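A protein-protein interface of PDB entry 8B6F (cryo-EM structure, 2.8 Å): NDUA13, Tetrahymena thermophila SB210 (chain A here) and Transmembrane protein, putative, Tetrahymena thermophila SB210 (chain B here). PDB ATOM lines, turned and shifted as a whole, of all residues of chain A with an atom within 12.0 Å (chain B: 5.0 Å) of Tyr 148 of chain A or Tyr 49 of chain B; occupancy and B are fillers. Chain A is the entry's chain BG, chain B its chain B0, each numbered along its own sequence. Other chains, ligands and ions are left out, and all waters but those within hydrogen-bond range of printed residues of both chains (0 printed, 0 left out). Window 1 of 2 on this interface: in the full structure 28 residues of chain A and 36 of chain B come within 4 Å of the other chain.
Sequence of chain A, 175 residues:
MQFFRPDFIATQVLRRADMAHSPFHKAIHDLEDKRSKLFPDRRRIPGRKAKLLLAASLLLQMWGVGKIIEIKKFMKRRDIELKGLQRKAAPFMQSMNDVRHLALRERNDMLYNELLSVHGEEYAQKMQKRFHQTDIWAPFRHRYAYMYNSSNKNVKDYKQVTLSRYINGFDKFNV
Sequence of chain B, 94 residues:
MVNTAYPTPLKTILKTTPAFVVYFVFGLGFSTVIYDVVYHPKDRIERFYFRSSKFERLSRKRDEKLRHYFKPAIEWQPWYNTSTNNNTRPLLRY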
ATOM      1  N   LEU A  82       3.078  25.788  29.216  1.00  0.00           N
ATOM      2  CA  LEU A  82       2.276  25.010  28.279  1.00  0.00           C
ATOM      3  C   LEU A  82       0.897  25.629  28.110  1.00  0.00           C
ATOM      4  O   LEU A  82       0.377  25.715  26.992  1.00  0.00           O
ATOM      5  CB  LEU A  82       2.155  23.558  28.744  1.00  0.00           C
ATOM      6  CG  LEU A  82       1.386  22.649  27.774  1.00  0.00           C
ATOM      7  CD1 LEU A  82       2.154  22.395  26.490  1.00  0.00           C
ATOM      8  CD2 LEU A  82       1.037  21.342  28.439  1.00  0.00           C
ATOM      9  N   GLN A  86      -0.852  27.059  24.715  1.00  0.00           N
ATOM     10  CA  GLN A  86      -2.190  26.628  24.325  1.00  0.00           C
ATOM     11  C   GLN A  86      -3.124  27.819  24.163  1.00  0.00           C
ATOM     12  O   GLN A  86      -3.962  27.844  23.255  1.00  0.00           O
ATOM     13  CB  GLN A  86      -2.742  25.639  25.352  1.00  0.00           C
ATOM     14  CG  GLN A  86      -2.000  24.312  25.376  1.00  0.00           C
ATOM     15  CD  GLN A  86      -2.462  23.407  26.496  1.00  0.00           C
ATOM     16  OE1 GLN A  86      -3.069  23.860  27.464  1.00  0.00           O
ATOM     17  NE2 GLN A  86      -2.182  22.117  26.365  1.00  0.00           N
ATOM     18  N   ARG A 143     -27.033  13.006  25.409  1.00  0.00           N
ATOM     19  CA  ARG A 143     -26.306  12.732  26.638  1.00  0.00           C
ATOM     20  C   ARG A 143     -25.066  13.608  26.661  1.00  0.00           C
ATOM     21  O   ARG A 143     -24.661  14.171  25.641  1.00  0.00           O
ATOM     22  CB  ARG A 143     -25.918  11.254  26.750  1.00  0.00           C
ATOM     23  CG  ARG A 143     -24.923  10.803  25.688  1.00  0.00           C
ATOM     24  CD  ARG A 143     -24.518   9.360  25.888  1.00  0.00           C
ATOM     25  NE  ARG A 143     -23.852   9.149  27.167  1.00  0.00           N
ATOM     26  CZ  ARG A 143     -22.547   9.273  27.367  1.00  0.00           C
ATOM     27  NH1 ARG A 143     -21.726   9.618  26.389  1.00  0.00           N
ATOM     28  NH2 ARG A 143     -22.053   9.046  28.579  1.00  0.00           N
ATOM     29  N   TYR A 144     -24.460  13.715  27.838  1.00  0.00           N
ATOM     30  CA  TYR A 144     -23.268  14.523  28.046  1.00  0.00           C
ATOM     31  C   TYR A 144     -22.072  13.611  28.279  1.00  0.00           C
ATOM     32  O   TYR A 144     -22.159  12.650  29.048  1.00  0.00           O
ATOM     33  CB  TYR A 144     -23.453  15.474  29.229  1.00  0.00           C
ATOM     34  CG  TYR A 144     -24.617  16.418  29.055  1.00  0.00           C
ATOM     35  CD1 TYR A 144     -25.912  16.014  29.347  1.00  0.00           C
ATOM     36  CD2 TYR A 144     -24.420  17.710  28.590  1.00  0.00           C
ATOM     37  CE1 TYR A 144     -26.979  16.871  29.187  1.00  0.00           C
ATOM     38  CE2 TYR A 144     -25.481  18.574  28.426  1.00  0.00           C
ATOM     39  CZ  TYR A 144     -26.758  18.149  28.727  1.00  0.00           C
ATOM     40  OH  TYR A 144     -27.818  19.007  28.563  1.00  0.00           O
ATOM     41  N   ALA A 145     -20.964  13.911  27.609  1.00  0.00           N
ATOM     42  CA  ALA A 145     -19.764  13.102  27.750  1.00  0.00           C
ATOM     43  C   ALA A 145     -19.214  13.203  29.166  1.00  0.00           C
ATOM     44  O   ALA A 145     -19.194  14.281  29.768  1.00  0.00           O
ATOM     45  CB  ALA A 145     -18.702  13.546  26.747  1.00  0.00           C
ATOM     46  N   TYR A 146     -18.770  12.068  29.701  1.00  0.00           N
ATOM     47  CA  TYR A 146     -18.172  12.007  31.028  1.00  0.00           C
ATOM     48  C   TYR A 146     -16.724  11.549  30.994  1.00  0.00           C
ATOM     49  O   TYR A 146     -15.852  12.225  31.552  1.00  0.00           O
ATOM     50  CB  TYR A 146     -18.994  11.075  31.928  1.00  0.00           C
ATOM     51  CG  TYR A 146     -18.277  10.662  33.191  1.00  0.00           C
ATOM     52  CD1 TYR A 146     -18.139  11.541  34.255  1.00  0.00           C
ATOM     53  CD2 TYR A 146     -17.751   9.387  33.325  1.00  0.00           C
ATOM     54  CE1 TYR A 146     -17.487  11.163  35.411  1.00  0.00           C
ATOM     55  CE2 TYR A 146     -17.099   9.000  34.475  1.00  0.00           C
ATOM     56  CZ  TYR A 146     -16.971   9.891  35.515  1.00  0.00           C
ATOM     57  OH  TYR A 146     -16.321   9.508  36.665  1.00  0.00           O
ATOM     58  N   MET A 147     -16.440  10.424  30.345  1.00  0.00           N
ATOM     59  CA  MET A 147     -15.102   9.856  30.373  1.00  0.00           C
ATOM     60  C   MET A 147     -14.102  10.773  29.680  1.00  0.00           C
ATOM     61  O   MET A 147     -14.444  11.539  28.776  1.00  0.00           O
ATOM     62  CB  MET A 147     -15.094   8.483  29.700  1.00  0.00           C
ATOM     63  CG  MET A 147     -15.453   7.323  30.615  1.00  0.00           C
ATOM     64  SD  MET A 147     -14.053   6.790  31.616  1.00  0.00           S
ATOM     65  CE  MET A 147     -14.425   7.576  33.177  1.00  0.00           C
ATOM     66  N   TYR A 148     -12.847  10.680  30.117  1.00  0.00           N
ATOM     67  CA  TYR A 148     -11.742  11.426  29.519  1.00  0.00           C
ATOM     68  C   TYR A 148     -12.015  12.927  29.538  1.00  0.00           C
ATOM     69  O   TYR A 148     -11.842  13.630  28.542  1.00  0.00           O
ATOM     70  CB  TYR A 148     -11.463  10.937  28.097  1.00  0.00           C
ATOM     71  CG  TYR A 148     -11.104   9.474  28.036  1.00  0.00           C
ATOM     72  CD1 TYR A 148      -9.838   9.036  28.395  1.00  0.00           C
ATOM     73  CD2 TYR A 148     -12.033   8.530  27.623  1.00  0.00           C
ATOM     74  CE1 TYR A 148      -9.505   7.699  28.346  1.00  0.00           C
ATOM     75  CE2 TYR A 148     -11.710   7.191  27.569  1.00  0.00           C
ATOM     76  CZ  TYR A 148     -10.445   6.781  27.932  1.00  0.00           C
ATOM     77  OH  TYR A 148     -10.117   5.447  27.879  1.00  0.00           O
ATOM     78  N   ASN A 149     -12.442  13.420  30.699  1.00  0.00           N
ATOM     79  CA  ASN A 149     -12.697  14.843  30.889  1.00  0.00           C
ATOM     80  C   ASN A 149     -13.716  15.354  29.872  1.00  0.00           C
ATOM     81  O   ASN A 149     -13.547  16.418  29.275  1.00  0.00           O
ATOM     82  CB  ASN A 149     -11.394  15.640  30.804  1.00  0.00           C
ATOM     83  CG  ASN A 149     -11.510  17.015  31.421  1.00  0.00           C
ATOM     84  OD1 ASN A 149     -12.576  17.627  31.408  1.00  0.00           O
ATOM     85  ND2 ASN A 149     -10.408  17.510  31.967  1.00  0.00           N
ATOM     86  N   SER A 150     -14.781  14.579  29.670  1.00  0.00           N
ATOM     87  CA  SER A 150     -15.833  14.908  28.711  1.00  0.00           C
ATOM     88  C   SER A 150     -15.254  15.034  27.302  1.00  0.00           C
ATOM     89  O   SER A 150     -15.366  16.066  26.639  1.00  0.00           O
ATOM     90  CB  SER A 150     -16.564  16.190  29.124  1.00  0.00           C
ATOM     91  OG  SER A 150     -17.286  15.998  30.328  1.00  0.00           O
ATOM     92  N   SER A 151     -14.623  13.951  26.858  1.00  0.00           N
ATOM     93  CA  SER A 151     -14.053  13.869  25.523  1.00  0.00           C
ATOM     94  C   SER A 151     -14.290  12.466  24.981  1.00  0.00           C
ATOM     95  O   SER A 151     -14.827  11.595  25.670  1.00  0.00           O
ATOM     96  CB  SER A 151     -12.563  14.214  25.535  1.00  0.00           C
ATOM     97  OG  SER A 151     -12.338  15.494  26.098  1.00  0.00           O
ATOM     98  N   ASN A 152     -13.889  12.252  23.731  1.00  0.00           N
ATOM     99  CA  ASN A 152     -14.017  10.959  23.068  1.00  0.00           C
ATOM    100  C   ASN A 152     -12.632  10.466  22.681  1.00  0.00           C
ATOM    101  O   ASN A 152     -11.946  11.101  21.873  1.00  0.00           O
ATOM    102  CB  ASN A 152     -14.915  11.060  21.835  1.00  0.00           C
ATOM    103  CG  ASN A 152     -16.360  11.329  22.192  1.00  0.00           C
ATOM    104  OD1 ASN A 152     -17.130  10.403  22.440  1.00  0.00           O
ATOM    105  ND2 ASN A 152     -16.735  12.602  22.222  1.00  0.00           N
ATOM    106  N   LYS A 153     -12.222   9.336  23.260  1.00  0.00           N
ATOM    107  CA  LYS A 153     -10.918   8.768  22.934  1.00  0.00           C
ATOM    108  C   LYS A 153     -10.906   8.194  21.523  1.00  0.00           C
ATOM    109  O   LYS A 153      -9.973   8.441  20.750  1.00  0.00           O
ATOM    110  CB  LYS A 153     -10.549   7.690  23.954  1.00  0.00           C
ATOM    111  CG  LYS A 153      -9.209   7.015  23.682  1.00  0.00           C
ATOM    112  CD  LYS A 153      -8.881   5.958  24.725  1.00  0.00           C
ATOM    113  CE  LYS A 153      -9.816   4.762  24.627  1.00  0.00           C
ATOM    114  NZ  LYS A 153      -9.434   3.678  25.576  1.00  0.00           N
ATOM    115  N   ASN A 154     -11.933   7.431  21.169  1.00  0.00           N
ATOM    116  CA  ASN A 154     -11.998   6.712  19.900  1.00  0.00           C
ATOM    117  C   ASN A 154     -13.041   7.384  19.012  1.00  0.00           C
ATOM    118  O   ASN A 154     -14.229   7.062  19.077  1.00  0.00           O
ATOM    119  CB  ASN A 154     -12.334   5.241  20.125  1.00  0.00           C
ATOM    120  CG  ASN A 154     -11.267   4.513  20.913  1.00  0.00           C
ATOM    121  OD1 ASN A 154     -11.524   3.997  21.999  1.00  0.00           O
ATOM    122  ND2 ASN A 154     -10.057   4.459  20.364  1.00  0.00           N
ATOM    123  N   VAL A 155     -12.595   8.322  18.185  1.00  0.00           N
ATOM    124  CA  VAL A 155     -13.471   8.928  17.169  1.00  0.00           C
ATOM    125  C   VAL A 155     -13.314   8.068  15.922  1.00  0.00           C
ATOM    126  O   VAL A 155     -12.609   8.403  14.968  1.00  0.00           O
ATOM    127  CB  VAL A 155     -13.132  10.400  16.918  1.00  0.00           C
ATOM    128  CG1 VAL A 155     -14.139  11.015  15.967  1.00  0.00           C
ATOM    129  CG2 VAL A 155     -13.078  11.170  18.229  1.00  0.00           C
ATOM    130  N   LYS A 156     -14.033   6.950  15.908  1.00  0.00           N
ATOM    131  CA  LYS A 156     -13.902   5.940  14.866  1.00  0.00           C
ATOM    132  C   LYS A 156     -15.065   4.970  15.008  1.00  0.00           C
ATOM    133  O   LYS A 156     -15.846   5.046  15.957  1.00  0.00           O
ATOM    134  CB  LYS A 156     -12.572   5.184  14.960  1.00  0.00           C
ATOM    135  CG  LYS A 156     -11.334   5.996  14.608  1.00  0.00           C
ATOM    136  CD  LYS A 156     -10.112   5.109  14.441  1.00  0.00           C
ATOM    137  CE  LYS A 156      -9.780   4.361  15.721  1.00  0.00           C
ATOM    138  NZ  LYS A 156      -9.555   5.272  16.876  1.00  0.00           N
ATOM    139  N   VAL A 161     -11.558   0.916  15.344  1.00  0.00           N
ATOM    140  CA  VAL A 161     -10.925   0.887  16.659  1.00  0.00           C
ATOM    141  C   VAL A 161     -10.192  -0.430  16.865  1.00  0.00           C
ATOM    142  O   VAL A 161      -9.073  -0.459  17.389  1.00  0.00           O
ATOM    143  CB  VAL A 161     -11.980   1.128  17.756  1.00  0.00           C
ATOM    144  CG1 VAL A 161     -11.442   0.756  19.131  1.00  0.00           C
ATOM    145  CG2 VAL A 161     -12.430   2.577  17.744  1.00  0.00           C
ATOM    146  N   SER A 164      -7.129  -0.703  13.817  1.00  0.00           N
ATOM    147  CA  SER A 164      -6.051   0.275  13.738  1.00  0.00           C
ATOM    148  C   SER A 164      -4.938  -0.004  14.738  1.00  0.00           C
ATOM    149  O   SER A 164      -3.829   0.513  14.570  1.00  0.00           O
ATOM    150  CB  SER A 164      -6.601   1.682  13.962  1.00  0.00           C
ATOM    151  OG  SER A 164      -7.283   1.767  15.198  1.00  0.00           O
ATOM    152  N   ARG A 165      -5.205  -0.794  15.779  1.00  0.00           N
ATOM    153  CA  ARG A 165      -4.161  -1.139  16.735  1.00  0.00           C
ATOM    154  C   ARG A 165      -3.176  -2.162  16.183  1.00  0.00           C
ATOM    155  O   ARG A 165      -2.112  -2.352  16.779  1.00  0.00           O
ATOM    156  CB  ARG A 165      -4.794  -1.668  18.025  1.00  0.00           C
ATOM    157  CG  ARG A 165      -3.839  -1.760  19.212  1.00  0.00           C
ATOM    158  CD  ARG A 165      -3.344  -0.388  19.648  1.00  0.00           C
ATOM    159  NE  ARG A 165      -2.518  -0.459  20.846  1.00  0.00           N
ATOM    160  CZ  ARG A 165      -1.900   0.579  21.395  1.00  0.00           C
ATOM    161  NH1 ARG A 165      -1.991   1.791  20.875  1.00  0.00           N
ATOM    162  NH2 ARG A 165      -1.175   0.396  22.494  1.00  0.00           N
ATOM    163  N   ASP A 171      -4.429   5.283  10.739  1.00  0.00           N
ATOM    164  CA  ASP A 171      -4.015   6.553  11.318  1.00  0.00           C
ATOM    165  C   ASP A 171      -3.551   7.500  10.221  1.00  0.00           C
ATOM    166  O   ASP A 171      -2.805   7.109   9.318  1.00  0.00           O
ATOM    167  CB  ASP A 171      -2.895   6.338  12.336  1.00  0.00           C
ATOM    168  CG  ASP A 171      -2.619   7.575  13.170  1.00  0.00           C
ATOM    169  OD1 ASP A 171      -3.335   8.583  12.996  1.00  0.00           O
ATOM    170  OD2 ASP A 171      -1.689   7.540  14.000  1.00  0.00           O
ATOM    171  N   ASN A 174      -1.632  13.292  11.856  1.00  0.00           N
ATOM    172  CA  ASN A 174      -2.147  14.659  11.896  1.00  0.00           C
ATOM    173  C   ASN A 174      -1.054  15.713  11.722  1.00  0.00           C
ATOM    174  O   ASN A 174      -1.343  16.912  11.749  1.00  0.00           O
ATOM    175  CB  ASN A 174      -2.876  14.913  13.219  1.00  0.00           C
ATOM    176  CG  ASN A 174      -4.129  14.075  13.366  1.00  0.00           C
ATOM    177  OD1 ASN A 174      -4.724  13.647  12.377  1.00  0.00           O
ATOM    178  ND2 ASN A 174      -4.542  13.845  14.606  1.00  0.00           N
ATOM    179  N   ARG B  47       1.595   8.505  22.452  1.00  0.00           N
ATOM    180  CA  ARG B  47       1.262   8.611  23.863  1.00  0.00           C
ATOM    181  C   ARG B  47      -0.207   8.278  24.084  1.00  0.00           C
ATOM    182  O   ARG B  47      -1.062   8.541  23.235  1.00  0.00           O
ATOM    183  CB  ARG B  47       1.571  10.016  24.383  1.00  0.00           C
ATOM    184  CG  ARG B  47       3.010  10.446  24.153  1.00  0.00           C
ATOM    185  CD  ARG B  47       3.369  11.695  24.945  1.00  0.00           C
ATOM    186  NE  ARG B  47       2.598  12.862  24.532  1.00  0.00           N
ATOM    187  CZ  ARG B  47       1.468  13.264  25.100  1.00  0.00           C
ATOM    188  NH1 ARG B  47       0.929  12.606  26.113  1.00  0.00           N
ATOM    189  NH2 ARG B  47       0.864  14.354  24.639  1.00  0.00           N
ATOM    190  N   PHE B  48      -0.498   7.684  25.238  1.00  0.00           N
ATOM    191  CA  PHE B  48      -1.876   7.349  25.562  1.00  0.00           C
ATOM    192  C   PHE B  48      -2.734   8.606  25.555  1.00  0.00           C
ATOM    193  O   PHE B  48      -2.286   9.699  25.905  1.00  0.00           O
ATOM    194  CB  PHE B  48      -1.966   6.669  26.930  1.00  0.00           C
ATOM    195  CG  PHE B  48      -1.413   5.268  26.965  1.00  0.00           C
ATOM    196  CD1 PHE B  48      -1.294   4.513  25.808  1.00  0.00           C
ATOM    197  CD2 PHE B  48      -1.024   4.704  28.167  1.00  0.00           C
ATOM    198  CE1 PHE B  48      -0.796   3.229  25.854  1.00  0.00           C
ATOM    199  CE2 PHE B  48      -0.525   3.421  28.217  1.00  0.00           C
ATOM    200  CZ  PHE B  48      -0.409   2.683  27.060  1.00  0.00           C
ATOM    201  N   TYR B  49      -3.989   8.435  25.141  1.00  0.00           N
ATOM    202  CA  TYR B  49      -4.892   9.574  25.043  1.00  0.00           C
ATOM    203  C   TYR B  49      -5.093  10.238  26.397  1.00  0.00           C
ATOM    204  O   TYR B  49      -5.073  11.470  26.502  1.00  0.00           O
ATOM    205  CB  TYR B  49      -6.228   9.116  24.463  1.00  0.00           C
ATOM    206  CG  TYR B  49      -7.249  10.214  24.353  1.00  0.00           C
ATOM    207  CD1 TYR B  49      -7.187  11.139  23.325  1.00  0.00           C
ATOM    208  CD2 TYR B  49      -8.286  10.316  25.266  1.00  0.00           C
ATOM    209  CE1 TYR B  49      -8.118  12.140  23.213  1.00  0.00           C
ATOM    210  CE2 TYR B  49      -9.224  11.313  25.163  1.00  0.00           C
ATOM    211  CZ  TYR B  49      -9.134  12.221  24.133  1.00  0.00           C
ATOM    212  OH  TYR B  49     -10.068  13.216  24.032  1.00  0.00           O
ATOM    213  N   PHE B  50      -5.278   9.441  27.451  1.00  0.00           N
ATOM    214  CA  PHE B  50      -5.517   9.993  28.778  1.00  0.00           C
ATOM    215  C   PHE B  50      -4.268  10.602  29.401  1.00  0.00           C
ATOM    216  O   PHE B  50      -4.386  11.321  30.398  1.00  0.00           O
ATOM    217  CB  PHE B  50      -6.080   8.913  29.703  1.00  0.00           C
ATOM    218  CG  PHE B  50      -5.216   7.693  29.811  1.00  0.00           C
ATOM    219  CD1 PHE B  50      -4.209   7.622  30.759  1.00  0.00           C
ATOM    220  CD2 PHE B  50      -5.417   6.610  28.970  1.00  0.00           C
ATOM    221  CE1 PHE B  50      -3.415   6.499  30.861  1.00  0.00           C
ATOM    222  CE2 PHE B  50      -4.628   5.485  29.067  1.00  0.00           C
ATOM    223  CZ  PHE B  50      -3.626   5.428  30.014  1.00  0.00           C
ATOM    224  N   ARG B  51      -3.089  10.338  28.848  1.00  0.00           N
ATOM    225  CA  ARG B  51      -1.856  10.977  29.304  1.00  0.00           C
ATOM    226  C   ARG B  51      -1.617  12.284  28.558  1.00  0.00           C
ATOM    227  O   ARG B  51      -0.550  12.510  27.991  1.00  0.00           O
ATOM    228  CB  ARG B  51      -0.676  10.031  29.120  1.00  0.00           C
ATOM    229  CG  ARG B  51      -0.775   8.735  29.900  1.00  0.00           C
ATOM    230  CD  ARG B  51      -0.709   8.955  31.402  1.00  0.00           C
ATOM    231  NE  ARG B  51       0.476   9.707  31.805  1.00  0.00           N
ATOM    232  CZ  ARG B  51       0.468  10.936  32.306  1.00  0.00           C
ATOM    233  NH1 ARG B  51      -0.660  11.601  32.508  1.00  0.00           N
ATOM    234  NH2 ARG B  51       1.622  11.511  32.626  1.00  0.00           N
ATOM    235  N   SER B  52      -2.618  13.159  28.552  1.00  0.00           N
ATOM    236  CA  SER B  52      -2.532  14.384  27.772  1.00  0.00           C
ATOM    237  C   SER B  52      -3.501  15.404  28.350  1.00  0.00           C
ATOM    238  O   SER B  52      -4.494  15.052  28.990  1.00  0.00           O
ATOM    239  CB  SER B  52      -2.839  14.115  26.295  1.00  0.00           C
ATOM    240  OG  SER B  52      -2.465  15.210  25.482  1.00  0.00           O
ATOM    241  N   LYS B  54      -6.319  18.551  28.300  1.00  0.00           N
ATOM    242  CA  LYS B  54      -7.596  18.684  27.607  1.00  0.00           C
ATOM    243  C   LYS B  54      -7.401  19.316  26.236  1.00  0.00           C
ATOM    244  O   LYS B  54      -7.940  18.835  25.234  1.00  0.00           O
ATOM    245  CB  LYS B  54      -8.564  19.509  28.455  1.00  0.00           C
ATOM    246  CG  LYS B  54      -9.961  19.646  27.868  1.00  0.00           C
ATOM    247  CD  LYS B  54     -10.696  18.318  27.842  1.00  0.00           C
ATOM    248  CE  LYS B  54     -12.124  18.485  27.345  1.00  0.00           C
ATOM    249  NZ  LYS B  54     -12.928  19.379  28.225  1.00  0.00           N
ATOM    250  N   ARG B  57      -5.743  16.846  23.896  1.00  0.00           N
ATOM    251  CA  ARG B  57      -6.700  15.845  23.436  1.00  0.00           C
ATOM    252  C   ARG B  57      -7.585  16.407  22.334  1.00  0.00           C
ATOM    253  O   ARG B  57      -7.816  15.751  21.311  1.00  0.00           O
ATOM    254  CB  ARG B  57      -7.556  15.370  24.609  1.00  0.00           C
ATOM    255  CG  ARG B  57      -6.795  14.613  25.681  1.00  0.00           C
ATOM    256  CD  ARG B  57      -7.591  14.575  26.973  1.00  0.00           C
ATOM    257  NE  ARG B  57      -6.862  13.926  28.053  1.00  0.00           N
ATOM    258  CZ  ARG B  57      -7.288  13.857  29.306  1.00  0.00           C
ATOM    259  NH1 ARG B  57      -8.436  14.399  29.676  1.00  0.00           N
ATOM    260  NH2 ARG B  57      -6.544  13.230  30.213  1.00  0.00           N
ATOM    261  N   ARG B  60      -5.596  16.724  19.120  1.00  0.00           N
ATOM    262  CA  ARG B  60      -5.315  15.422  18.523  1.00  0.00           C
ATOM    263  C   ARG B  60      -6.538  14.851  17.816  1.00  0.00           C
ATOM    264  O   ARG B  60      -6.421  14.303  16.714  1.00  0.00           O
ATOM    265  CB  ARG B  60      -4.826  14.455  19.602  1.00  0.00           C
ATOM    266  CG  ARG B  60      -3.460  14.804  20.170  1.00  0.00           C
ATOM    267  CD  ARG B  60      -3.178  14.054  21.463  1.00  0.00           C
ATOM    268  NE  ARG B  60      -2.947  12.631  21.242  1.00  0.00           N
ATOM    269  CZ  ARG B  60      -2.674  11.760  22.203  1.00  0.00           C
ATOM    270  NH1 ARG B  60      -2.598  12.129  23.471  1.00  0.00           N
ATOM    271  NH2 ARG B  60      -2.474  10.484  21.884  1.00  0.00           N
ATOM    272  N   LYS B  61      -7.716  14.967  18.427  1.00  0.00           N
ATOM    273  CA  LYS B  61      -8.917  14.336  17.898  1.00  0.00           C
ATOM    274  C   LYS B  61      -9.709  15.228  16.953  1.00  0.00           C
ATOM    275  O   LYS B  61     -10.691  14.759  16.371  1.00  0.00           O
ATOM    276  CB  LYS B  61      -9.824  13.892  19.049  1.00  0.00           C
ATOM    277  CG  LYS B  61      -9.174  12.895  19.996  1.00  0.00           C
ATOM    278  CD  LYS B  61      -8.839  11.587  19.290  1.00  0.00           C
ATOM    279  CE  LYS B  61      -8.090  10.642  20.211  1.00  0.00           C
ATOM    280  NZ  LYS B  61      -7.778   9.350  19.543  1.00  0.00           N
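CB of Tyr 148 of chain A touches CE2 of Tyr 49 of chain B, 3.7 Å away.
Phe 50 of chain B touches Tyr 148 of chain A (CB to CE1, 3.9 Å).
Tyr 148 of chain A touches Arg 57 of chain B.
CB of Asn 149 of chain A touches NH1 of Arg 57 of chain B, 3.4 Å away.
CB of Ser 151 of chain A touches OH of Tyr 49 of chain B, 3.1 Å away.
CE of Lys 54 of chain B touches OG of Ser 151 of chain A, at 3.2 Å.
Asn 152 of chain A touches Tyr 49 of chain B (O to OH, 3.6 Å).
Asn 152 of chain A touches Lys 61 of chain B (O to CG, 3.8 Å).
Lys 153 of chain A touches Tyr 49 of chain B (CB to CD2, 3.7 Å).
The backbone carbonyl oxygen of Asn 149 of chain A lies close to the side-chain amino group of Lys 54 of chain B.
The backbone carbonyl oxygen (O) of Arg 60 of chain B sits at hydrogen-bond distance from the side-chain amide nitrogen (ND2) of Asn 174 of chain A (2.9 Å).
NZ of Lys 61 of chain B lies within hydrogen-bond range of O of Lys 153 of chain A, at 2.7 Å.
Printed residues of chain A that touch a printed residue of chain B: Tyr 148, Asn 149, Ser 151, Asn 152, Lys 153 and Asn 174.
Hydrophobic or aromatic side chains of chain A within 4 Å of the printed part of chain B: Tyr 148.
Along chain A the printed residues that touch a printed residue of chain B span positions 148 to 174.
The backbone carbonyl oxygen (O) of Phe 48 of chain B sits at hydrogen-bond distance from the guanidinium group (NH1) of Arg 60 of chain B (3.5 Å).
O of Tyr 49 of chain B lies within hydrogen-bond range of NE of Arg 57 of chain B (3.4 Å).
NH2 of Arg 57 of chain B sits at hydrogen-bond distance from O of Phe 50 of chain B.
The guanidinium group of Arg 57 of chain B is in hydrogen-bond range of the backbone carbonyl oxygen of Ser 52 of chain B (2.8 Å).
The backbone carbonyl oxygen (O) of Tyr 148 of chain A lies within hydrogen-bond range of the side-chain hydroxyl (OG) of Ser 151 of chain A (3.1 Å).
NZ of Lys 153 of chain A lies within hydrogen-bond range of OH of Tyr 148 of chain A, at 3.0 Å.
Tyr 148 of chain A touches just these residues of chain B: Tyr 49 (3.7 Å), Phe 50 (3.9 Å) and Arg 57 (3.7 Å).
Arg 57 of chain B touches just these residues of chain A: Tyr 148 and Asn 149.
Of chain A, only Asn 174 (2.9 Å) comes within 4 Å of Arg 60 of chain B.
Lys 61 of chain B touches just these residues of chain A: Asn 152 and Lys 153.
Of the printed residues of chain B, Lys 153 of chain A touches Tyr 49 (3.7 Å) and Lys 61 (2.7 Å).
Of the printed residues of chain B, Asn 149 of chain A touches Lys 54 (3.2 Å) and Arg 57 (3.4 Å).
Printed residues of chain B within 4 Å of Asn 152 of chain A: Tyr 49 and Lys 61.
Printed residues of chain B within 4 Å of Asn 174 of chain A: Arg 60 (2.9 Å).
Printed residues of chain B within 4 Å of Ser 151 of chain A: Tyr 49 and Lys 54.
Tyr 144 of chain A touches none of the printed residues of chain B.
Ala 145 of chain A touches none of the printed residues of chain B.
The nearest residue of chain A that does not touch Tyr 49 of chain B is Asn 154 of chain A (6.2 Å).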
